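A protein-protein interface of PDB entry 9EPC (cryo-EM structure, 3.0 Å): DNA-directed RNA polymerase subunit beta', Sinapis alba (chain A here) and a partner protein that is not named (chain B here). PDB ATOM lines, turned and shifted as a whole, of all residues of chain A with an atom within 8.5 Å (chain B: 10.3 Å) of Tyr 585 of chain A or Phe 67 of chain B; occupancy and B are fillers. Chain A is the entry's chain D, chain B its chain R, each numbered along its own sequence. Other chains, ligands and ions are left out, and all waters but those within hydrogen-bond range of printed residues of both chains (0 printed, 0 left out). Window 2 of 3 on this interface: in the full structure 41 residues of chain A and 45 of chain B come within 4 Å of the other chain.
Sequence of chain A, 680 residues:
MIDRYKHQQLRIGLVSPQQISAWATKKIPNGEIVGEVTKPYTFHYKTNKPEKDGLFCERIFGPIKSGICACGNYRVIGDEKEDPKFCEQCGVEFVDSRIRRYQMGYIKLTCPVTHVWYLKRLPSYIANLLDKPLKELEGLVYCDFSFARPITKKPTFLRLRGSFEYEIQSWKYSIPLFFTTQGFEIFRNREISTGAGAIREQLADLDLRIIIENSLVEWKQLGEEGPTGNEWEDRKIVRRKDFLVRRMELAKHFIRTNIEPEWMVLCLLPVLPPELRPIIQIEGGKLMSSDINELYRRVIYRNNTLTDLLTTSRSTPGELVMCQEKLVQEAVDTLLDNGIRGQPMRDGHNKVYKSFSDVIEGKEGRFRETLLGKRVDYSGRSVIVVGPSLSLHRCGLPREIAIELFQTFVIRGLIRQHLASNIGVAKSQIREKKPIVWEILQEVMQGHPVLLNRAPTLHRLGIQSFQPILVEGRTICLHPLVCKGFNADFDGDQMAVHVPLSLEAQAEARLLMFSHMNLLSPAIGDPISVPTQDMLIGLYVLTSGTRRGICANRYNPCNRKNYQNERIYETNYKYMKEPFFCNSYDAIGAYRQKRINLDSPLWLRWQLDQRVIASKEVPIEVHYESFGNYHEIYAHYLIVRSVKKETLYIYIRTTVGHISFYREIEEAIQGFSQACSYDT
The guanidinium group (NH2) of Arg 64 of chain B lies close to the side-chain amide nitrogen (NE2) of Gln 674 of chain A, at 3.1 Å.
The side-chain amide oxygen (OE1) of Gln 71 of chain B lies close to the backbone carbonyl oxygen (O) of Glu 667 of chain A (2.8 Å).
The guanidinium group of Arg 663 of chain A is in salt-bridge range of the side-chain carboxylate of Glu 667 of chain A, 2.9 Å away.
Among the printed residues, merely in contact across the chains: Tyr 585 of chain A with Pro 66 of chain B, Tyr 585 of chain A with Phe 67 of chain B, Glu 667 of chain A with Val 68 of chain B, Ala 668 of chain A with Gln 71 of chain B, Gln 670 of chain A with Val 65 of chain B, Gly 671 of chain A with Val 68 of chain B, Gly 671 of chain A with Gln 71 of chain B, Gly 671 of chain A with Val 72 of chain B, Gln 674 of chain A with Val 68 of chain B and Gln 674 of chain A with Val 72 of chain B.
Ser 584 of chain A touches none of the printed residues of chain B.
No residue of chain B comes within 4 Å of Asp 586 of chain A.
No residue of chain B comes within 4 Å of Ala 587 of chain A.
No residue of chain B comes within 4 Å of Ile 588 of chain A.
No residue of chain B comes within 4 Å of Gly 589 of chain A.
Arg 592 of chain A touches none of the printed residues of chain B.
Leu 604 of chain A touches none of the printed residues of chain B.
Printed residues of chain B within 4 Å of Gly 671 of chain A: Val 68 (3.9 Å), Gln 71 (3.7 Å) and Val 72 (3.3 Å).
Of the printed residues of chain A, Arg 64 of chain B touches Gln 674 (3.1 Å).
Of the printed residues of chain A, Val 65 of chain B touches Gln 670 (3.5 Å).
Pro 66 of chain B touches just one residue of chain A: Tyr 585.
Of chain A, only Tyr 585 comes within 4 Å of Phe 67 of chain B.
Printed residues of chain A within 4 Å of Val 68 of chain B: Glu 667, Gly 671 and Gln 674.
Printed residues of chain A within 4 Å of Gln 71 of chain B: Glu 667, Ala 668 and Gly 671.
The nearest residue of chain B that does not touch Tyr 585 of chain A is Val 65 of chain B (4.1 Å).
The nearest residue of chain A that does not touch Phe 67 of chain B is Glu 667 of chain A (4.03 Å).
The nearest printed residue of chain A that does not touch Val 72 of chain B is Gln 670 of chain A (5.0 Å).
Printed residues of chain A that touch a printed residue of chain B: Tyr 585, Glu 667, Ala 668, Gln 670, Gly 671 and Gln 674.
Hydrophobic or aromatic side chains of chain B within 4 Å of the printed part of chain A: Val 65, Pro 66, Phe 67, Val 68 and Val 72.
Among the printed residues, no Asp or Glu carboxylate lies within 4 Å of a Lys or Arg side-chain nitrogen of the other chain.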
ATOM      1  N   PHE A 581     -14.528 -20.474  18.947  1.00  0.00           N
ATOM      2  CA  PHE A 581     -13.412 -19.544  19.028  1.00  0.00           C
ATOM      3  C   PHE A 581     -13.378 -18.912  20.410  1.00  0.00           C
ATOM      4  O   PHE A 581     -14.395 -18.402  20.890  1.00  0.00           O
ATOM      5  CB  PHE A 581     -13.517 -18.470  17.946  1.00  0.00           C
ATOM      6  CG  PHE A 581     -13.393 -19.009  16.557  1.00  0.00           C
ATOM      7  CD1 PHE A 581     -12.155 -19.342  16.042  1.00  0.00           C
ATOM      8  CD2 PHE A 581     -14.511 -19.192  15.767  1.00  0.00           C
ATOM      9  CE1 PHE A 581     -12.035 -19.843  14.767  1.00  0.00           C
ATOM     10  CE2 PHE A 581     -14.394 -19.693  14.490  1.00  0.00           C
ATOM     11  CZ  PHE A 581     -13.155 -20.019  13.990  1.00  0.00           C
ATOM     12  N   CYS A 582     -12.207 -18.952  21.046  1.00  0.00           N
ATOM     13  CA  CYS A 582     -12.070 -18.420  22.394  1.00  0.00           C
ATOM     14  C   CYS A 582     -12.192 -16.904  22.439  1.00  0.00           C
ATOM     15  O   CYS A 582     -12.564 -16.357  23.481  1.00  0.00           O
ATOM     16  CB  CYS A 582     -10.734 -18.856  22.989  1.00  0.00           C
ATOM     17  SG  CYS A 582      -9.310 -18.460  21.956  1.00  0.00           S
ATOM     18  N   ASN A 583     -11.888 -16.216  21.341  1.00  0.00           N
ATOM     19  CA  ASN A 583     -12.003 -14.767  21.296  1.00  0.00           C
ATOM     20  C   ASN A 583     -12.212 -14.334  19.855  1.00  0.00           C
ATOM     21  O   ASN A 583     -11.968 -15.093  18.915  1.00  0.00           O
ATOM     22  CB  ASN A 583     -10.771 -14.083  21.895  1.00  0.00           C
ATOM     23  CG  ASN A 583      -9.478 -14.695  21.415  1.00  0.00           C
ATOM     24  OD1 ASN A 583      -9.465 -15.470  20.462  1.00  0.00           O
ATOM     25  ND2 ASN A 583      -8.379 -14.352  22.074  1.00  0.00           N
ATOM     26  N   SER A 584     -12.671 -13.092  19.693  1.00  0.00           N
ATOM     27  CA  SER A 584     -13.001 -12.593  18.365  1.00  0.00           C
ATOM     28  C   SER A 584     -11.775 -12.500  17.469  1.00  0.00           C
ATOM     29  O   SER A 584     -11.897 -12.576  16.243  1.00  0.00           O
ATOM     30  CB  SER A 584     -13.681 -11.231  18.476  1.00  0.00           C
ATOM     31  OG  SER A 584     -12.849 -10.306  19.152  1.00  0.00           O
ATOM     32  N   TYR A 585     -10.588 -12.330  18.055  1.00  0.00           N
ATOM     33  CA  TYR A 585      -9.381 -12.219  17.244  1.00  0.00           C
ATOM     34  C   TYR A 585      -9.096 -13.516  16.498  1.00  0.00           C
ATOM     35  O   TYR A 585      -8.674 -13.487  15.336  1.00  0.00           O
ATOM     36  CB  TYR A 585      -8.196 -11.826  18.122  1.00  0.00           C
ATOM     37  CG  TYR A 585      -8.480 -10.634  19.002  1.00  0.00           C
ATOM     38  CD1 TYR A 585      -8.648  -9.370  18.457  1.00  0.00           C
ATOM     39  CD2 TYR A 585      -8.585 -10.773  20.378  1.00  0.00           C
ATOM     40  CE1 TYR A 585      -8.911  -8.277  19.257  1.00  0.00           C
ATOM     41  CE2 TYR A 585      -8.847  -9.688  21.187  1.00  0.00           C
ATOM     42  CZ  TYR A 585      -9.009  -8.442  20.622  1.00  0.00           C
ATOM     43  OH  TYR A 585      -9.271  -7.357  21.425  1.00  0.00           O
ATOM     44  N   ASP A 586      -9.311 -14.660  17.148  1.00  0.00           N
ATOM     45  CA  ASP A 586      -9.126 -15.936  16.466  1.00  0.00           C
ATOM     46  C   ASP A 586     -10.148 -16.122  15.355  1.00  0.00           C
ATOM     47  O   ASP A 586      -9.820 -16.650  14.286  1.00  0.00           O
ATOM     48  CB  ASP A 586      -9.205 -17.086  17.465  1.00  0.00           C
ATOM     49  CG  ASP A 586      -8.030 -17.109  18.414  1.00  0.00           C
ATOM     50  OD1 ASP A 586      -7.252 -16.134  18.417  1.00  0.00           O
ATOM     51  OD2 ASP A 586      -7.880 -18.103  19.154  1.00  0.00           O
ATOM     52  N   ALA A 587     -11.393 -15.702  15.588  1.00  0.00           N
ATOM     53  CA  ALA A 587     -12.410 -15.805  14.548  1.00  0.00           C
ATOM     54  C   ALA A 587     -12.038 -14.968  13.334  1.00  0.00           C
ATOM     55  O   ALA A 587     -12.190 -15.414  12.193  1.00  0.00           O
ATOM     56  CB  ALA A 587     -13.770 -15.381  15.098  1.00  0.00           C
ATOM     57  N   ILE A 588     -11.550 -13.747  13.560  1.00  0.00           N
ATOM     58  CA  ILE A 588     -11.082 -12.920  12.453  1.00  0.00           C
ATOM     59  C   ILE A 588      -9.869 -13.557  11.792  1.00  0.00           C
ATOM     60  O   ILE A 588      -9.774 -13.617  10.561  1.00  0.00           O
ATOM     61  CB  ILE A 588     -10.773 -11.494  12.941  1.00  0.00           C
ATOM     62  CG1 ILE A 588     -12.030 -10.840  13.511  1.00  0.00           C
ATOM     63  CG2 ILE A 588     -10.209 -10.659  11.809  1.00  0.00           C
ATOM     64  CD1 ILE A 588     -13.136 -10.683  12.506  1.00  0.00           C
ATOM     65  N   GLY A 589      -8.926 -14.043  12.599  1.00  0.00           N
ATOM     66  CA  GLY A 589      -7.729 -14.648  12.042  1.00  0.00           C
ATOM     67  C   GLY A 589      -8.024 -15.894  11.231  1.00  0.00           C
ATOM     68  O   GLY A 589      -7.437 -16.107  10.168  1.00  0.00           O
ATOM     69  N   ALA A 590      -8.937 -16.735  11.719  1.00  0.00           N
ATOM     70  CA  ALA A 590      -9.325 -17.919  10.963  1.00  0.00           C
ATOM     71  C   ALA A 590      -9.977 -17.534   9.643  1.00  0.00           C
ATOM     72  O   ALA A 590      -9.779 -18.206   8.624  1.00  0.00           O
ATOM     73  CB  ALA A 590     -10.267 -18.788  11.792  1.00  0.00           C
ATOM     74  N   TYR A 591     -10.761 -16.455   9.644  1.00  0.00           N
ATOM     75  CA  TYR A 591     -11.369 -15.982   8.405  1.00  0.00           C
ATOM     76  C   TYR A 591     -10.311 -15.519   7.414  1.00  0.00           C
ATOM     77  O   TYR A 591     -10.438 -15.753   6.207  1.00  0.00           O
ATOM     78  CB  TYR A 591     -12.354 -14.856   8.703  1.00  0.00           C
ATOM     79  CG  TYR A 591     -12.836 -14.128   7.475  1.00  0.00           C
ATOM     80  CD1 TYR A 591     -13.641 -14.761   6.542  1.00  0.00           C
ATOM     81  CD2 TYR A 591     -12.493 -12.804   7.253  1.00  0.00           C
ATOM     82  CE1 TYR A 591     -14.086 -14.099   5.422  1.00  0.00           C
ATOM     83  CE2 TYR A 591     -12.933 -12.134   6.135  1.00  0.00           C
ATOM     84  CZ  TYR A 591     -13.730 -12.786   5.222  1.00  0.00           C
ATOM     85  OH  TYR A 591     -14.173 -12.121   4.104  1.00  0.00           O
ATOM     86  N   ARG A 592      -9.263 -14.852   7.901  1.00  0.00           N
ATOM     87  CA  ARG A 592      -8.183 -14.431   7.017  1.00  0.00           C
ATOM     88  C   ARG A 592      -7.482 -15.632   6.398  1.00  0.00           C
ATOM     89  O   ARG A 592      -7.116 -15.607   5.218  1.00  0.00           O
ATOM     90  CB  ARG A 592      -7.184 -13.565   7.781  1.00  0.00           C
ATOM     91  CG  ARG A 592      -7.748 -12.244   8.252  1.00  0.00           C
ATOM     92  CD  ARG A 592      -6.794 -11.555   9.204  1.00  0.00           C
ATOM     93  NE  ARG A 592      -7.386 -10.358   9.787  1.00  0.00           N
ATOM     94  CZ  ARG A 592      -6.867  -9.687  10.805  1.00  0.00           C
ATOM     95  NH1 ARG A 592      -5.741 -10.073  11.384  1.00  0.00           N
ATOM     96  NH2 ARG A 592      -7.494  -8.606  11.258  1.00  0.00           N
ATOM     97  N   LEU A 604     -18.701 -18.057  19.490  1.00  0.00           N
ATOM     98  CA  LEU A 604     -17.738 -17.130  20.062  1.00  0.00           C
ATOM     99  C   LEU A 604     -17.861 -17.177  21.577  1.00  0.00           C
ATOM    100  O   LEU A 604     -18.946 -16.948  22.119  1.00  0.00           O
ATOM    101  CB  LEU A 604     -17.979 -15.713  19.549  1.00  0.00           C
ATOM    102  CG  LEU A 604     -16.950 -14.666  19.965  1.00  0.00           C
ATOM    103  CD1 LEU A 604     -15.602 -15.001  19.367  1.00  0.00           C
ATOM    104  CD2 LEU A 604     -17.403 -13.283  19.540  1.00  0.00           C
ATOM    105  N   VAL A 656     -18.404 -14.209  11.257  1.00  0.00           N
ATOM    106  CA  VAL A 656     -17.296 -13.262  11.214  1.00  0.00           C
ATOM    107  C   VAL A 656     -17.803 -11.872  10.862  1.00  0.00           C
ATOM    108  O   VAL A 656     -17.296 -10.864  11.368  1.00  0.00           O
ATOM    109  CB  VAL A 656     -16.220 -13.743  10.224  1.00  0.00           C
ATOM    110  CG1 VAL A 656     -15.113 -12.719  10.101  1.00  0.00           C
ATOM    111  CG2 VAL A 656     -15.655 -15.069  10.674  1.00  0.00           C
ATOM    112  N   ILE A 659     -19.020 -10.137  13.880  1.00  0.00           N
ATOM    113  CA  ILE A 659     -17.846  -9.841  14.691  1.00  0.00           C
ATOM    114  C   ILE A 659     -17.049  -8.700  14.077  1.00  0.00           C
ATOM    115  O   ILE A 659     -16.608  -7.783  14.779  1.00  0.00           O
ATOM    116  CB  ILE A 659     -16.985 -11.105  14.862  1.00  0.00           C
ATOM    117  CG1 ILE A 659     -17.728 -12.139  15.703  1.00  0.00           C
ATOM    118  CG2 ILE A 659     -15.656 -10.759  15.494  1.00  0.00           C
ATOM    119  CD1 ILE A 659     -16.998 -13.447  15.826  1.00  0.00           C
ATOM    120  N   ARG A 663     -16.464  -5.347  15.957  1.00  0.00           N
ATOM    121  CA  ARG A 663     -15.087  -4.980  16.259  1.00  0.00           C
ATOM    122  C   ARG A 663     -14.718  -3.642  15.637  1.00  0.00           C
ATOM    123  O   ARG A 663     -13.943  -2.879  16.223  1.00  0.00           O
ATOM    124  CB  ARG A 663     -14.135  -6.072  15.774  1.00  0.00           C
ATOM    125  CG  ARG A 663     -13.336  -6.737  16.877  1.00  0.00           C
ATOM    126  CD  ARG A 663     -12.226  -7.591  16.298  1.00  0.00           C
ATOM    127  NE  ARG A 663     -11.042  -6.798  15.990  1.00  0.00           N
ATOM    128  CZ  ARG A 663     -10.471  -6.739  14.794  1.00  0.00           C
ATOM    129  NH1 ARG A 663     -11.116  -7.112  13.701  1.00  0.00           N
ATOM    130  NH2 ARG A 663      -9.223  -6.294  14.693  1.00  0.00           N
ATOM    131  N   GLU A 666     -16.070  -0.944  17.934  1.00  0.00           N
ATOM    132  CA  GLU A 666     -15.336  -0.929  19.194  1.00  0.00           C
ATOM    133  C   GLU A 666     -13.918  -0.407  19.002  1.00  0.00           C
ATOM    134  O   GLU A 666     -13.424   0.378  19.818  1.00  0.00           O
ATOM    135  CB  GLU A 666     -15.315  -2.328  19.804  1.00  0.00           C
ATOM    136  CG  GLU A 666     -14.711  -2.385  21.193  1.00  0.00           C
ATOM    137  CD  GLU A 666     -14.618  -3.799  21.729  1.00  0.00           C
ATOM    138  OE1 GLU A 666     -14.594  -4.746  20.914  1.00  0.00           O
ATOM    139  OE2 GLU A 666     -14.573  -3.967  22.965  1.00  0.00           O
ATOM    140  N   GLU A 667     -13.244  -0.834  17.933  1.00  0.00           N
ATOM    141  CA  GLU A 667     -11.893  -0.346  17.674  1.00  0.00           C
ATOM    142  C   GLU A 667     -11.892   1.145  17.360  1.00  0.00           C
ATOM    143  O   GLU A 667     -10.969   1.865  17.758  1.00  0.00           O
ATOM    144  CB  GLU A 667     -11.253  -1.129  16.531  1.00  0.00           C
ATOM    145  CG  GLU A 667     -10.776  -2.515  16.919  1.00  0.00           C
ATOM    146  CD  GLU A 667      -9.982  -3.184  15.815  1.00  0.00           C
ATOM    147  OE1 GLU A 667      -9.780  -2.548  14.759  1.00  0.00           O
ATOM    148  OE2 GLU A 667      -9.558  -4.343  16.003  1.00  0.00           O
ATOM    149  N   ALA A 668     -12.908   1.624  16.641  1.00  0.00           N
ATOM    150  CA  ALA A 668     -12.987   3.047  16.337  1.00  0.00           C
ATOM    151  C   ALA A 668     -13.094   3.874  17.609  1.00  0.00           C
ATOM    152  O   ALA A 668     -12.467   4.933  17.726  1.00  0.00           O
ATOM    153  CB  ALA A 668     -14.175   3.323  15.419  1.00  0.00           C
ATOM    154  N   GLN A 670     -12.103   2.920  20.733  1.00  0.00           N
ATOM    155  CA  GLN A 670     -10.846   2.815  21.465  1.00  0.00           C
ATOM    156  C   GLN A 670      -9.734   3.583  20.766  1.00  0.00           C
ATOM    157  O   GLN A 670      -8.918   4.241  21.422  1.00  0.00           O
ATOM    158  CB  GLN A 670     -10.456   1.352  21.636  1.00  0.00           C
ATOM    159  CG  GLN A 670     -11.499   0.505  22.333  1.00  0.00           C
ATOM    160  CD  GLN A 670     -11.763   0.957  23.750  1.00  0.00           C
ATOM    161  OE1 GLN A 670     -10.903   1.555  24.396  1.00  0.00           O
ATOM    162  NE2 GLN A 670     -12.962   0.674  24.246  1.00  0.00           N
ATOM    163  N   GLY A 671      -9.675   3.502  19.437  1.00  0.00           N
ATOM    164  CA  GLY A 671      -8.659   4.244  18.710  1.00  0.00           C
ATOM    165  C   GLY A 671      -8.804   5.742  18.879  1.00  0.00           C
ATOM    166  O   GLY A 671      -7.813   6.465  18.980  1.00  0.00           O
ATOM    167  N   GLN A 674      -7.690   6.576  22.606  1.00  0.00           N
ATOM    168  CA  GLN A 674      -6.247   6.565  22.819  1.00  0.00           C
ATOM    169  C   GLN A 674      -5.578   7.770  22.171  1.00  0.00           C
ATOM    170  O   GLN A 674      -4.654   8.356  22.745  1.00  0.00           O
ATOM    171  CB  GLN A 674      -5.642   5.270  22.285  1.00  0.00           C
ATOM    172  CG  GLN A 674      -6.024   4.036  23.072  1.00  0.00           C
ATOM    173  CD  GLN A 674      -5.208   2.827  22.673  1.00  0.00           C
ATOM    174  OE1 GLN A 674      -4.191   2.950  21.991  1.00  0.00           O
ATOM    175  NE2 GLN A 674      -5.649   1.649  23.096  1.00  0.00           N
ATOM    176  N   GLN B  63     -10.307  -4.219  30.072  1.00  0.00           N
ATOM    177  CA  GLN B  63      -9.549  -4.678  28.917  1.00  0.00           C
ATOM    178  C   GLN B  63      -9.389  -3.564  27.889  1.00  0.00           C
ATOM    179  O   GLN B  63     -10.235  -2.675  27.762  1.00  0.00           O
ATOM    180  CB  GLN B  63     -10.228  -5.885  28.267  1.00  0.00           C
ATOM    181  CG  GLN B  63     -10.026  -7.196  29.011  1.00  0.00           C
ATOM    182  CD  GLN B  63     -10.824  -7.272  30.294  1.00  0.00           C
ATOM    183  OE1 GLN B  63     -11.775  -6.516  30.493  1.00  0.00           O
ATOM    184  NE2 GLN B  63     -10.442  -8.187  31.176  1.00  0.00           N
ATOM    185  N   ARG B  64      -8.285  -3.627  27.149  1.00  0.00           N
ATOM    186  CA  ARG B  64      -7.976  -2.670  26.096  1.00  0.00           C
ATOM    187  C   ARG B  64      -7.679  -3.419  24.806  1.00  0.00           C
ATOM    188  O   ARG B  64      -6.990  -4.445  24.820  1.00  0.00           O
ATOM    189  CB  ARG B  64      -6.782  -1.788  26.481  1.00  0.00           C
ATOM    190  CG  ARG B  64      -5.617  -2.558  27.081  1.00  0.00           C
ATOM    191  CD  ARG B  64      -4.416  -1.661  27.338  1.00  0.00           C
ATOM    192  NE  ARG B  64      -3.750  -1.267  26.103  1.00  0.00           N
ATOM    193  CZ  ARG B  64      -3.927  -0.103  25.493  1.00  0.00           C
ATOM    194  NH1 ARG B  64      -4.745   0.815  25.981  1.00  0.00           N
ATOM    195  NH2 ARG B  64      -3.263   0.147  24.368  1.00  0.00           N
ATOM    196  N   VAL B  65      -8.202  -2.907  23.697  1.00  0.00           N
ATOM    197  CA  VAL B  65      -8.007  -3.539  22.395  1.00  0.00           C
ATOM    198  C   VAL B  65      -6.542  -3.397  21.996  1.00  0.00           C
ATOM    199  O   VAL B  65      -5.900  -2.390  22.329  1.00  0.00           O
ATOM    200  CB  VAL B  65      -8.944  -2.943  21.334  1.00  0.00           C
ATOM    201  CG1 VAL B  65     -10.392  -3.047  21.790  1.00  0.00           C
ATOM    202  CG2 VAL B  65      -8.572  -1.505  21.049  1.00  0.00           C
ATOM    203  N   PRO B  66      -5.967  -4.385  21.319  1.00  0.00           N
ATOM    204  CA  PRO B  66      -4.531  -4.339  21.024  1.00  0.00           C
ATOM    205  C   PRO B  66      -4.175  -3.848  19.628  1.00  0.00           C
ATOM    206  O   PRO B  66      -2.992  -3.648  19.337  1.00  0.00           O
ATOM    207  CB  PRO B  66      -4.104  -5.798  21.221  1.00  0.00           C
ATOM    208  CG  PRO B  66      -5.383  -6.619  21.031  1.00  0.00           C
ATOM    209  CD  PRO B  66      -6.554  -5.675  20.931  1.00  0.00           C
ATOM    210  N   PHE B  67      -5.161  -3.647  18.755  1.00  0.00           N
ATOM    211  CA  PHE B  67      -4.847  -3.422  17.348  1.00  0.00           C
ATOM    212  C   PHE B  67      -5.330  -2.072  16.838  1.00  0.00           C
ATOM    213  O   PHE B  67      -5.919  -1.991  15.755  1.00  0.00           O
ATOM    214  CB  PHE B  67      -5.446  -4.535  16.488  1.00  0.00           C
ATOM    215  CG  PHE B  67      -5.016  -5.909  16.895  1.00  0.00           C
ATOM    216  CD1 PHE B  67      -3.702  -6.310  16.747  1.00  0.00           C
ATOM    217  CD2 PHE B  67      -5.927  -6.806  17.417  1.00  0.00           C
ATOM    218  CE1 PHE B  67      -3.306  -7.574  17.118  1.00  0.00           C
ATOM    219  CE2 PHE B  67      -5.535  -8.072  17.787  1.00  0.00           C
ATOM    220  CZ  PHE B  67      -4.223  -8.456  17.639  1.00  0.00           C
ATOM    221  N   VAL B  68      -5.084  -1.007  17.593  1.00  0.00           N
ATOM    222  CA  VAL B  68      -5.473   0.331  17.175  1.00  0.00           C
ATOM    223  C   VAL B  68      -4.256   1.224  16.944  1.00  0.00           C
ATOM    224  O   VAL B  68      -4.380   2.441  16.919  1.00  0.00           O
ATOM    225  CB  VAL B  68      -6.448   0.965  18.183  1.00  0.00           C
ATOM    226  CG1 VAL B  68      -7.825   0.352  18.034  1.00  0.00           C
ATOM    227  CG2 VAL B  68      -5.933   0.777  19.598  1.00  0.00           C
ATOM    228  N   GLU B  69      -3.075   0.626  16.773  1.00  0.00           N
ATOM    229  CA  GLU B  69      -1.873   1.421  16.542  1.00  0.00           C
ATOM    230  C   GLU B  69      -1.973   2.208  15.243  1.00  0.00           C
ATOM    231  O   GLU B  69      -1.552   3.369  15.177  1.00  0.00           O
ATOM    232  CB  GLU B  69      -0.637   0.522  16.525  1.00  0.00           C
ATOM    233  CG  GLU B  69      -0.231  -0.022  17.882  1.00  0.00           C
ATOM    234  CD  GLU B  69      -1.111  -1.162  18.348  1.00  0.00           C
ATOM    235  OE1 GLU B  69      -1.975  -1.609  17.566  1.00  0.00           O
ATOM    236  OE2 GLU B  69      -0.937  -1.615  19.498  1.00  0.00           O
ATOM    237  N   GLU B  70      -2.516   1.590  14.194  1.00  0.00           N
ATOM    238  CA  GLU B  70      -2.650   2.288  12.922  1.00  0.00           C
ATOM    239  C   GLU B  70      -3.752   3.338  12.969  1.00  0.00           C
ATOM    240  O   GLU B  70      -3.663   4.356  12.274  1.00  0.00           O
ATOM    241  CB  GLU B  70      -2.911   1.288  11.795  1.00  0.00           C
ATOM    242  CG  GLU B  70      -4.196   0.478  11.932  1.00  0.00           C
ATOM    243  CD  GLU B  70      -4.067  -0.699  12.886  1.00  0.00           C
ATOM    244  OE1 GLU B  70      -3.567  -0.511  14.014  1.00  0.00           O
ATOM    245  OE2 GLU B  70      -4.468  -1.818  12.502  1.00  0.00           O
ATOM    246  N   GLN B  71      -4.797   3.111  13.768  1.00  0.00           N
ATOM    247  CA  GLN B  71      -5.859   4.103  13.886  1.00  0.00           C
ATOM    248  C   GLN B  71      -5.375   5.346  14.620  1.00  0.00           C
ATOM    249  O   GLN B  71      -5.585   6.472  14.156  1.00  0.00           O
ATOM    250  CB  GLN B  71      -7.069   3.504  14.598  1.00  0.00           C
ATOM    251  CG  GLN B  71      -7.897   2.569  13.746  1.00  0.00           C
ATOM    252  CD  GLN B  71      -9.212   2.219  14.401  1.00  0.00           C
ATOM    253  OE1 GLN B  71      -9.543   2.740  15.465  1.00  0.00           O
ATOM    254  NE2 GLN B  71      -9.972   1.333  13.771  1.00  0.00           N
ATOM    255  N   VAL B  72      -4.719   5.162  15.768  1.00  0.00           N
ATOM    256  CA  VAL B  72      -4.293   6.311  16.561  1.00  0.00           C
ATOM    257  C   VAL B  72      -3.254   7.128  15.803  1.00  0.00           C
ATOM    258  O   VAL B  72      -3.227   8.359  15.898  1.00  0.00           O
ATOM    259  CB  VAL B  72      -3.777   5.859  17.940  1.00  0.00           C
ATOM    260  CG1 VAL B  72      -4.867   5.122  18.692  1.00  0.00           C
ATOM    261  CG2 VAL B  72      -2.544   4.986  17.807  1.00  0.00           C
ATOM    262  N   ARG B  73      -2.388   6.460  15.039  1.00  0.00           N
ATOM    263  CA  ARG B  73      -1.429   7.185  14.215  1.00  0.00           C
ATOM    264  C   ARG B  73      -2.129   7.945  13.098  1.00  0.00           C
ATOM    265  O   ARG B  73      -1.762   9.086  12.791  1.00  0.00           O
ATOM    266  CB  ARG B  73      -0.396   6.218  13.644  1.00  0.00           C
ATOM    267  CG  ARG B  73       0.630   6.874  12.745  1.00  0.00           C
ATOM    268  CD  ARG B  73       1.663   5.876  12.261  1.00  0.00           C
ATOM    269  NE  ARG B  73       1.071   4.822  11.446  1.00  0.00           N
ATOM    270  CZ  ARG B  73       0.798   3.600  11.882  1.00  0.00           C
ATOM    271  NH1 ARG B  73       1.062   3.234  13.126  1.00  0.00           N
ATOM    272  NH2 ARG B  73       0.249   2.722  11.049  1.00  0.00           N
ATOM    273  N   LYS B  74      -3.132   7.328  12.475  1.00  0.00           N
ATOM    274  CA  LYS B  74      -3.875   8.003  11.417  1.00  0.00           C
ATOM    275  C   LYS B  74      -4.641   9.203  11.958  1.00  0.00           C
ATOM    276  O   LYS B  74      -4.686  10.257  11.315  1.00  0.00           O
ATOM    277  CB  LYS B  74      -4.827   7.021  10.738  1.00  0.00           C
ATOM    278  CG  LYS B  74      -5.542   7.582   9.524  1.00  0.00           C
ATOM    279  CD  LYS B  74      -4.561   7.911   8.413  1.00  0.00           C
ATOM    280  CE  LYS B  74      -5.281   8.349   7.148  1.00  0.00           C
ATOM    281  NZ  LYS B  74      -6.173   7.281   6.616  1.00  0.00           N
